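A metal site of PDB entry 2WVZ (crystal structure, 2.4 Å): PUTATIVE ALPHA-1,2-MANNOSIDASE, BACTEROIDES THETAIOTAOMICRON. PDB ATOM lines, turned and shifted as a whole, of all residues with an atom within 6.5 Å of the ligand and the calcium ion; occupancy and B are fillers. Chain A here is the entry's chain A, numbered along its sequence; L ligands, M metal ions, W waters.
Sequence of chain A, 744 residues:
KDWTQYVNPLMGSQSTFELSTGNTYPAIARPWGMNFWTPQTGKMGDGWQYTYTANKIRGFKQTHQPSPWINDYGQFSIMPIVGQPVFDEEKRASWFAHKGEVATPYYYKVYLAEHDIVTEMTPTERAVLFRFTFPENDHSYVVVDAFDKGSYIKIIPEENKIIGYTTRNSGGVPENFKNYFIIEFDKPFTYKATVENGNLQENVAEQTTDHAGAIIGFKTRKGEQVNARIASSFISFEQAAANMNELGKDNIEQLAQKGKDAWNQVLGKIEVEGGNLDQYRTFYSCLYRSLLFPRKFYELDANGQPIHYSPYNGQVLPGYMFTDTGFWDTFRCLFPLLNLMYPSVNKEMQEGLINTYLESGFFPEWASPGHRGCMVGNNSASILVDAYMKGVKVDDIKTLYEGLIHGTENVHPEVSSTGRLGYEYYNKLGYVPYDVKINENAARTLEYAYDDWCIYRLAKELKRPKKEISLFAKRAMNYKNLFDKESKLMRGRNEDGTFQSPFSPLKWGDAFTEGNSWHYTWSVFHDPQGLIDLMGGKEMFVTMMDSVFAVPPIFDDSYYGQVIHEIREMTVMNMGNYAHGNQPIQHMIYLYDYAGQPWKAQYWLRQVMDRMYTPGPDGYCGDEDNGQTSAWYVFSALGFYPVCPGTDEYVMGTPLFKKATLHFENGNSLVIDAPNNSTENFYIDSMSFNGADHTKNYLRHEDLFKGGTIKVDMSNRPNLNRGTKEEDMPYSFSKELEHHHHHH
An oxygen (O3) of the ligand sits close to the side-chain carboxylate of Glu 514 (2.5 Å). OD1 of Asp 329 lies within hydrogen-bond range of O1 of the ligand (2.5 Å). The indole nitrogen of Trp 366 sits at hydrogen-bond distance from an oxygen (O1) of the ligand. OG of Ser 67 is in hydrogen-bond range of O6 of the ligand (2.8 Å). A nitrogen (N1) of the ligand lies within hydrogen-bond range of the side-chain carboxylate (OE2) of Glu 566 (3.4 Å). An oxygen (O5) of the ligand is in hydrogen-bond range of the side-chain sulfur (SG) of Cys 374 (3.6 Å).
A ring nitrogen (NE2) of His 565 sits at hydrogen-bond distance from the side-chain carboxylate of Glu 566, 3.0 Å away. The backbone NH of Trp 69 lies close to the side-chain hydroxyl of Ser 67. The side-chain carboxylate (OD2) of Asp 329 lies close to the side-chain amide oxygen (OE1) of Gln 583. The side-chain amide nitrogen (NE2) of Gln 583 is in hydrogen-bond range of the side-chain hydroxyl (OG1) of Thr 629 (3.2 Å). The side-chain amide nitrogen (ND2) of Asn 582 is in hydrogen-bond range of the side-chain carboxylate (OE2) of Glu 514, at 3.1 Å. The indole nitrogen of Trp 69 sits at hydrogen-bond distance from the side-chain carboxylate of Asp 623, at 2.8 Å. OG of Ser 67 sits at hydrogen-bond distance from N of Ile 70. The indole nitrogen of Trp 366 lies close to the side-chain sulfur of Cys 374 (3.7 Å).
Trp 69 touches the ligand. CG1 of Ile 70 touches C8 of the ligand (3.7 Å). CZ3 of Trp 328 touches O2 of the ligand (3.4 Å). Met 375 touches the ligand (SD to C3, 3.8 Å). The nearest printed residue that does not touch the ligand is Asp 623 (4.3 Å).
Within 4 Å of the calcium ion: Asn 582, Gln 583 and Asp 625. Along chain A the residues within 4 Å of the calcium ion span positions 582 to 625. The nearest printed residue that does not touch the calcium ion is Asp 623 (4.2 Å).
The calcium ion is bound by OD1 of Asn 582, O3 of the ligand, O2 of the ligand, water W2, water W1, OD2 of Asp 625 and OE1 of Gln 583. The calcium ion has seven donor atoms within binding distance.
Water W2 lies within hydrogen-bond range of NE2 of Gln 583 (2.8 Å), O of Gly 581 (2.8 Å) and O of Asp 623 (3.0 Å). Water W1 bridges the side-chain carboxylate of Glu 566 (3.0 Å) and the side-chain carboxylate of Asp 623 (3.4 Å). Water W3 lies within hydrogen-bond range of the side-chain carboxylate (OD1) of Asp 625 (2.7 Å), an oxygen (O6) of the ligand (2.7 Å) and the side-chain amide oxygen (OD1) of Asn 626 (3.2 Å).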
ATOM      1  N   PRO A  66     -12.936  28.838  36.582  1.00  0.00           N
ATOM      2  CA  PRO A  66     -12.284  27.542  36.324  1.00  0.00           C
ATOM      3  C   PRO A  66     -11.001  27.625  35.438  1.00  0.00           C
ATOM      4  O   PRO A  66     -10.229  26.671  35.414  1.00  0.00           O
ATOM      5  CB  PRO A  66     -13.361  26.735  35.591  1.00  0.00           C
ATOM      6  CG  PRO A  66     -14.341  27.760  35.047  1.00  0.00           C
ATOM      7  CD  PRO A  66     -14.036  29.124  35.642  1.00  0.00           C
ATOM      8  N   SER A  67     -10.794  28.731  34.714  1.00  0.00           N
ATOM      9  CA  SER A  67      -9.578  28.883  33.889  1.00  0.00           C
ATOM     10  C   SER A  67      -9.502  30.300  33.373  1.00  0.00           C
ATOM     11  O   SER A  67     -10.544  30.958  33.236  1.00  0.00           O
ATOM     12  CB  SER A  67      -9.601  27.947  32.687  1.00  0.00           C
ATOM     13  OG  SER A  67     -10.531  28.421  31.683  1.00  0.00           O
ATOM     14  N   PRO A  68      -8.290  30.772  33.012  1.00  0.00           N
ATOM     15  CA  PRO A  68      -8.138  32.112  32.415  1.00  0.00           C
ATOM     16  C   PRO A  68      -8.892  32.216  31.069  1.00  0.00           C
ATOM     17  O   PRO A  68      -9.224  33.319  30.619  1.00  0.00           O
ATOM     18  CB  PRO A  68      -6.625  32.254  32.217  1.00  0.00           C
ATOM     19  CG  PRO A  68      -6.124  30.871  32.107  1.00  0.00           C
ATOM     20  CD  PRO A  68      -7.026  30.006  32.960  1.00  0.00           C
ATOM     21  N   TRP A  69      -9.215  31.071  30.462  1.00  0.00           N
ATOM     22  CA  TRP A  69      -9.959  31.051  29.197  1.00  0.00           C
ATOM     23  C   TRP A  69     -11.456  31.191  29.421  1.00  0.00           C
ATOM     24  O   TRP A  69     -12.099  31.993  28.777  1.00  0.00           O
ATOM     25  CB  TRP A  69      -9.629  29.801  28.381  1.00  0.00           C
ATOM     26  CG  TRP A  69      -8.145  29.544  28.365  1.00  0.00           C
ATOM     27  CD1 TRP A  69      -7.476  28.537  29.003  1.00  0.00           C
ATOM     28  CD2 TRP A  69      -7.143  30.356  27.737  1.00  0.00           C
ATOM     29  NE1 TRP A  69      -6.123  28.649  28.773  1.00  0.00           N
ATOM     30  CE2 TRP A  69      -5.892  29.758  28.006  1.00  0.00           C
ATOM     31  CE3 TRP A  69      -7.184  31.514  26.934  1.00  0.00           C
ATOM     32  CZ2 TRP A  69      -4.697  30.271  27.521  1.00  0.00           C
ATOM     33  CZ3 TRP A  69      -5.989  32.027  26.449  1.00  0.00           C
ATOM     34  CH2 TRP A  69      -4.759  31.400  26.746  1.00  0.00           C
ATOM     35  N   ILE A  70     -12.010  30.446  30.352  1.00  0.00           N
ATOM     36  CA  ILE A  70     -13.404  30.543  30.674  1.00  0.00           C
ATOM     37  C   ILE A  70     -13.730  31.861  31.375  1.00  0.00           C
ATOM     38  O   ILE A  70     -14.774  32.457  31.115  1.00  0.00           O
ATOM     39  CB  ILE A  70     -13.853  29.336  31.540  1.00  0.00           C
ATOM     40  CG1 ILE A  70     -13.774  28.054  30.698  1.00  0.00           C
ATOM     41  CG2 ILE A  70     -15.252  29.514  32.053  1.00  0.00           C
ATOM     42  CD1 ILE A  70     -14.815  28.006  29.578  1.00  0.00           C
ATOM     43  N   GLY A 326     -15.210  21.307  32.430  1.00  0.00           N
ATOM     44  CA  GLY A 326     -15.368  20.974  31.029  1.00  0.00           C
ATOM     45  C   GLY A 326     -15.114  19.499  30.829  1.00  0.00           C
ATOM     46  O   GLY A 326     -13.999  19.062  30.950  1.00  0.00           O
ATOM     47  N   TRP A 328     -14.554  17.704  28.537  1.00  0.00           N
ATOM     48  CA  TRP A 328     -13.618  17.374  27.485  1.00  0.00           C
ATOM     49  C   TRP A 328     -12.264  17.144  28.112  1.00  0.00           C
ATOM     50  O   TRP A 328     -11.472  16.319  27.627  1.00  0.00           O
ATOM     51  CB  TRP A 328     -13.571  18.498  26.443  1.00  0.00           C
ATOM     52  CG  TRP A 328     -12.558  18.286  25.358  1.00  0.00           C
ATOM     53  CD1 TRP A 328     -12.762  17.659  24.153  1.00  0.00           C
ATOM     54  CD2 TRP A 328     -11.196  18.748  25.334  1.00  0.00           C
ATOM     55  NE1 TRP A 328     -11.609  17.687  23.400  1.00  0.00           N
ATOM     56  CE2 TRP A 328     -10.642  18.350  24.103  1.00  0.00           C
ATOM     57  CE3 TRP A 328     -10.395  19.442  26.246  1.00  0.00           C
ATOM     58  CZ2 TRP A 328      -9.303  18.623  23.760  1.00  0.00           C
ATOM     59  CZ3 TRP A 328      -9.069  19.737  25.888  1.00  0.00           C
ATOM     60  CH2 TRP A 328      -8.542  19.328  24.665  1.00  0.00           C
ATOM     61  N   ASP A 329     -11.993  17.889  29.181  1.00  0.00           N
ATOM     62  CA  ASP A 329     -10.820  17.642  30.030  1.00  0.00           C
ATOM     63  C   ASP A 329     -11.115  16.464  30.956  1.00  0.00           C
ATOM     64  O   ASP A 329     -10.419  15.466  30.915  1.00  0.00           O
ATOM     65  CB  ASP A 329     -10.502  18.841  30.939  1.00  0.00           C
ATOM     66  CG  ASP A 329     -10.210  20.116  30.177  1.00  0.00           C
ATOM     67  OD1 ASP A 329     -10.852  21.159  30.477  1.00  0.00           O
ATOM     68  OD2 ASP A 329      -9.331  20.075  29.302  1.00  0.00           O
ATOM     69  N   TRP A 366     -19.249  21.835  28.676  1.00  0.00           N
ATOM     70  CA  TRP A 366     -18.577  22.854  29.460  1.00  0.00           C
ATOM     71  C   TRP A 366     -19.672  23.664  30.183  1.00  0.00           C
ATOM     72  O   TRP A 366     -20.683  24.048  29.587  1.00  0.00           O
ATOM     73  CB  TRP A 366     -17.725  23.762  28.582  1.00  0.00           C
ATOM     74  CG  TRP A 366     -16.309  23.743  28.965  1.00  0.00           C
ATOM     75  CD1 TRP A 366     -15.267  23.281  28.220  1.00  0.00           C
ATOM     76  CD2 TRP A 366     -15.749  24.157  30.218  1.00  0.00           C
ATOM     77  NE1 TRP A 366     -14.096  23.400  28.921  1.00  0.00           N
ATOM     78  CE2 TRP A 366     -14.363  23.940  30.150  1.00  0.00           C
ATOM     79  CE3 TRP A 366     -16.283  24.698  31.395  1.00  0.00           C
ATOM     80  CZ2 TRP A 366     -13.500  24.237  31.204  1.00  0.00           C
ATOM     81  CZ3 TRP A 366     -15.428  24.985  32.443  1.00  0.00           C
ATOM     82  CH2 TRP A 366     -14.051  24.742  32.345  1.00  0.00           C
ATOM     83  N   CYS A 374     -17.458  26.023  24.393  1.00  0.00           N
ATOM     84  CA  CYS A 374     -16.043  25.726  24.566  1.00  0.00           C
ATOM     85  C   CYS A 374     -15.759  24.248  24.392  1.00  0.00           C
ATOM     86  O   CYS A 374     -16.406  23.435  25.008  1.00  0.00           O
ATOM     87  CB  CYS A 374     -15.599  26.130  25.978  1.00  0.00           C
ATOM     88  SG  CYS A 374     -13.830  25.972  26.225  1.00  0.00           S
ATOM     89  N   MET A 375     -14.761  23.921  23.568  1.00  0.00           N
ATOM     90  CA  MET A 375     -14.299  22.556  23.301  1.00  0.00           C
ATOM     91  C   MET A 375     -15.294  21.706  22.544  1.00  0.00           C
ATOM     92  O   MET A 375     -16.208  22.241  21.901  1.00  0.00           O
ATOM     93  CB  MET A 375     -13.823  21.843  24.566  1.00  0.00           C
ATOM     94  CG  MET A 375     -12.716  22.574  25.339  1.00  0.00           C
ATOM     95  SD  MET A 375     -11.452  23.527  24.405  1.00  0.00           S
ATOM     96  CE  MET A 375     -10.418  22.199  23.740  1.00  0.00           C
ATOM     97  N   GLU A 514      -6.889  21.680  19.104  1.00  0.00           N
ATOM     98  CA  GLU A 514      -5.664  21.984  19.840  1.00  0.00           C
ATOM     99  C   GLU A 514      -4.694  20.798  19.844  1.00  0.00           C
ATOM    100  O   GLU A 514      -4.162  20.403  20.893  1.00  0.00           O
ATOM    101  CB  GLU A 514      -6.003  22.441  21.247  1.00  0.00           C
ATOM    102  CG  GLU A 514      -6.922  23.671  21.317  1.00  0.00           C
ATOM    103  CD  GLU A 514      -7.388  23.977  22.731  1.00  0.00           C
ATOM    104  OE1 GLU A 514      -8.312  24.812  22.904  1.00  0.00           O
ATOM    105  OE2 GLU A 514      -6.829  23.376  23.686  1.00  0.00           O
ATOM    106  N   HIS A 565       0.022  28.758  23.000  1.00  0.00           N
ATOM    107  CA  HIS A 565       0.833  28.234  24.079  1.00  0.00           C
ATOM    108  C   HIS A 565       0.907  26.705  24.074  1.00  0.00           C
ATOM    109  O   HIS A 565       1.948  26.169  24.398  1.00  0.00           O
ATOM    110  CB  HIS A 565       0.368  28.762  25.430  1.00  0.00           C
ATOM    111  CG  HIS A 565      -0.992  28.311  25.813  1.00  0.00           C
ATOM    112  ND1 HIS A 565      -1.219  27.193  26.591  1.00  0.00           N
ATOM    113  CD2 HIS A 565      -2.212  28.817  25.522  1.00  0.00           C
ATOM    114  CE1 HIS A 565      -2.522  27.041  26.770  1.00  0.00           C
ATOM    115  NE2 HIS A 565      -3.142  28.010  26.134  1.00  0.00           N
ATOM    116  N   GLU A 566      -0.176  26.008  23.693  1.00  0.00           N
ATOM    117  CA  GLU A 566      -0.157  24.518  23.641  1.00  0.00           C
ATOM    118  C   GLU A 566       0.916  24.044  22.674  1.00  0.00           C
ATOM    119  O   GLU A 566       1.577  23.045  22.931  1.00  0.00           O
ATOM    120  CB  GLU A 566      -1.509  23.899  23.260  1.00  0.00           C
ATOM    121  CG  GLU A 566      -2.647  24.034  24.301  1.00  0.00           C
ATOM    122  CD  GLU A 566      -3.383  25.363  24.186  1.00  0.00           C
ATOM    123  OE1 GLU A 566      -2.901  26.211  23.395  1.00  0.00           O
ATOM    124  OE2 GLU A 566      -4.423  25.551  24.868  1.00  0.00           O
ATOM    125  N   GLY A 581       1.191  18.391  27.655  1.00  0.00           N
ATOM    126  CA  GLY A 581       0.507  19.610  28.086  1.00  0.00           C
ATOM    127  C   GLY A 581      -0.953  19.726  27.686  1.00  0.00           C
ATOM    128  O   GLY A 581      -1.662  20.613  28.186  1.00  0.00           O
ATOM    129  N   ASN A 582      -1.428  18.854  26.793  1.00  0.00           N
ATOM    130  CA  ASN A 582      -2.823  18.917  26.444  1.00  0.00           C
ATOM    131  C   ASN A 582      -3.486  17.554  26.474  1.00  0.00           C
ATOM    132  O   ASN A 582      -2.858  16.533  26.158  1.00  0.00           O
ATOM    133  CB  ASN A 582      -3.067  19.686  25.145  1.00  0.00           C
ATOM    134  CG  ASN A 582      -4.302  20.601  25.225  1.00  0.00           C
ATOM    135  OD1 ASN A 582      -4.751  20.966  26.328  1.00  0.00           O
ATOM    136  ND2 ASN A 582      -4.853  20.987  24.065  1.00  0.00           N
ATOM    137  N   GLN A 583      -4.772  17.562  26.840  1.00  0.00           N
ATOM    138  CA  GLN A 583      -5.514  16.378  27.276  1.00  0.00           C
ATOM    139  C   GLN A 583      -5.592  15.233  26.289  1.00  0.00           C
ATOM    140  O   GLN A 583      -5.673  14.075  26.710  1.00  0.00           O
ATOM    141  CB  GLN A 583      -6.956  16.749  27.633  1.00  0.00           C
ATOM    142  CG  GLN A 583      -7.118  17.523  28.897  1.00  0.00           C
ATOM    143  CD  GLN A 583      -6.295  18.769  28.874  1.00  0.00           C
ATOM    144  OE1 GLN A 583      -6.335  19.566  27.921  1.00  0.00           O
ATOM    145  NE2 GLN A 583      -5.507  18.962  29.933  1.00  0.00           N
ATOM    146  N   PRO A 584      -5.609  15.535  24.984  1.00  0.00           N
ATOM    147  CA  PRO A 584      -6.009  14.476  24.048  1.00  0.00           C
ATOM    148  C   PRO A 584      -5.023  13.298  24.016  1.00  0.00           C
ATOM    149  O   PRO A 584      -5.430  12.165  23.831  1.00  0.00           O
ATOM    150  CB  PRO A 584      -6.094  15.189  22.694  1.00  0.00           C
ATOM    151  CG  PRO A 584      -5.975  16.672  22.991  1.00  0.00           C
ATOM    152  CD  PRO A 584      -5.303  16.815  24.310  1.00  0.00           C
ATOM    153  N   GLY A 622       1.758  22.419  31.179  1.00  0.00           N
ATOM    154  CA  GLY A 622       0.604  22.931  30.428  1.00  0.00           C
ATOM    155  C   GLY A 622      -0.529  23.277  31.365  1.00  0.00           C
ATOM    156  O   GLY A 622      -0.353  23.288  32.578  1.00  0.00           O
ATOM    157  N   ASP A 623      -1.705  23.567  30.829  1.00  0.00           N
ATOM    158  CA  ASP A 623      -2.803  23.936  31.690  1.00  0.00           C
ATOM    159  C   ASP A 623      -3.209  22.783  32.613  1.00  0.00           C
ATOM    160  O   ASP A 623      -3.135  21.601  32.259  1.00  0.00           O
ATOM    161  CB  ASP A 623      -3.991  24.409  30.865  1.00  0.00           C
ATOM    162  CG  ASP A 623      -3.794  25.814  30.285  1.00  0.00           C
ATOM    163  OD1 ASP A 623      -2.667  26.358  30.322  1.00  0.00           O
ATOM    164  OD2 ASP A 623      -4.765  26.384  29.796  1.00  0.00           O
ATOM    165  N   GLU A 624      -3.661  23.130  33.817  1.00  0.00           N
ATOM    166  CA  GLU A 624      -4.080  22.122  34.786  1.00  0.00           C
ATOM    167  C   GLU A 624      -5.478  21.547  34.476  1.00  0.00           C
ATOM    168  O   GLU A 624      -5.729  20.329  34.599  1.00  0.00           O
ATOM    169  CB  GLU A 624      -4.055  22.726  36.184  1.00  0.00           C
ATOM    170  CG  GLU A 624      -4.013  21.735  37.273  1.00  0.00           C
ATOM    171  CD  GLU A 624      -5.352  21.150  37.578  1.00  0.00           C
ATOM    172  OE1 GLU A 624      -6.339  21.914  37.550  1.00  0.00           O
ATOM    173  OE2 GLU A 624      -5.422  19.932  37.854  1.00  0.00           O
ATOM    174  N   ASP A 625      -6.378  22.447  34.109  1.00  0.00           N
ATOM    175  CA  ASP A 625      -7.708  22.116  33.649  1.00  0.00           C
ATOM    176  C   ASP A 625      -8.513  21.317  34.642  1.00  0.00           C
ATOM    177  O   ASP A 625      -8.937  20.188  34.359  1.00  0.00           O
ATOM    178  CB  ASP A 625      -7.652  21.392  32.315  1.00  0.00           C
ATOM    179  CG  ASP A 625      -7.128  22.274  31.194  1.00  0.00           C
ATOM    180  OD1 ASP A 625      -7.471  23.499  31.137  1.00  0.00           O
ATOM    181  OD2 ASP A 625      -6.366  21.741  30.357  1.00  0.00           O
ATOM    182  N   ASN A 626      -8.732  21.922  35.800  1.00  0.00           N
ATOM    183  CA  ASN A 626      -9.774  21.475  36.719  1.00  0.00           C
ATOM    184  C   ASN A 626      -9.694  20.063  37.243  1.00  0.00           C
ATOM    185  O   ASN A 626     -10.721  19.438  37.542  1.00  0.00           O
ATOM    186  CB  ASN A 626     -11.112  21.765  36.091  1.00  0.00           C
ATOM    187  CG  ASN A 626     -11.175  23.178  35.591  1.00  0.00           C
ATOM    188  OD1 ASN A 626     -11.417  23.416  34.426  1.00  0.00           O
ATOM    189  ND2 ASN A 626     -10.888  24.120  36.473  1.00  0.00           N
ATOM    190  N   THR A 629      -5.096  17.335  34.491  1.00  0.00           N
ATOM    191  CA  THR A 629      -3.657  17.185  34.323  1.00  0.00           C
ATOM    192  C   THR A 629      -2.999  16.727  35.639  1.00  0.00           C
ATOM    193  O   THR A 629      -1.925  16.090  35.641  1.00  0.00           O
ATOM    194  CB  THR A 629      -3.087  18.522  33.839  1.00  0.00           C
ATOM    195  OG1 THR A 629      -3.798  18.912  32.661  1.00  0.00           O
ATOM    196  CG2 THR A 629      -1.586  18.429  33.550  1.00  0.00           C
HETATM  197  C1  LIG L   1     -10.074  23.766  28.485  1.00  0.00           C
HETATM  198  O1  LIG L   1     -11.197  22.970  28.792  1.00  0.00           O
HETATM  199  C2  LIG L   1      -9.160  22.984  27.498  1.00  0.00           C
HETATM  200  O2  LIG L   1      -8.254  22.117  28.233  1.00  0.00           O
HETATM  201  C3  LIG L   1      -8.374  23.945  26.569  1.00  0.00           C
HETATM  202  O3  LIG L   1      -7.134  23.362  26.175  1.00  0.00           O
HETATM  203  C4  LIG L   1      -8.173  25.308  27.241  1.00  0.00           C
HETATM  204  N1  LIG L   1      -7.389  26.223  26.339  1.00  0.00           N
HETATM  205  C5  LIG L   1      -8.253  27.081  25.759  1.00  0.00           C
HETATM  206  O4  LIG L   1      -7.986  27.971  24.940  1.00  0.00           O
HETATM  207  C6  LIG L   1      -9.547  26.850  26.243  1.00  0.00           C
HETATM  208  O5  LIG L   1     -10.538  27.476  25.869  1.00  0.00           O
HETATM  209  N2  LIG L   1      -9.537  25.830  27.218  1.00  0.00           N
HETATM  210  C7  LIG L   1     -10.609  25.101  27.911  1.00  0.00           C
HETATM  211  C8  LIG L   1     -11.280  25.971  28.966  1.00  0.00           C
HETATM  212  O6  LIG L   1     -10.280  26.302  29.906  1.00  0.00           O
HETATM  213 CA    CA M   1      -5.811  22.180  27.820  1.00  0.00          CA
HETATM  214  O   HOH W   1      -3.976  23.989  27.447  1.00  0.00           O
HETATM  215  O   HOH W   2      -4.062  21.256  29.462  1.00  0.00           O
HETATM  216  O   HOH W   3      -9.894  24.424  31.858  1.00  0.00           O
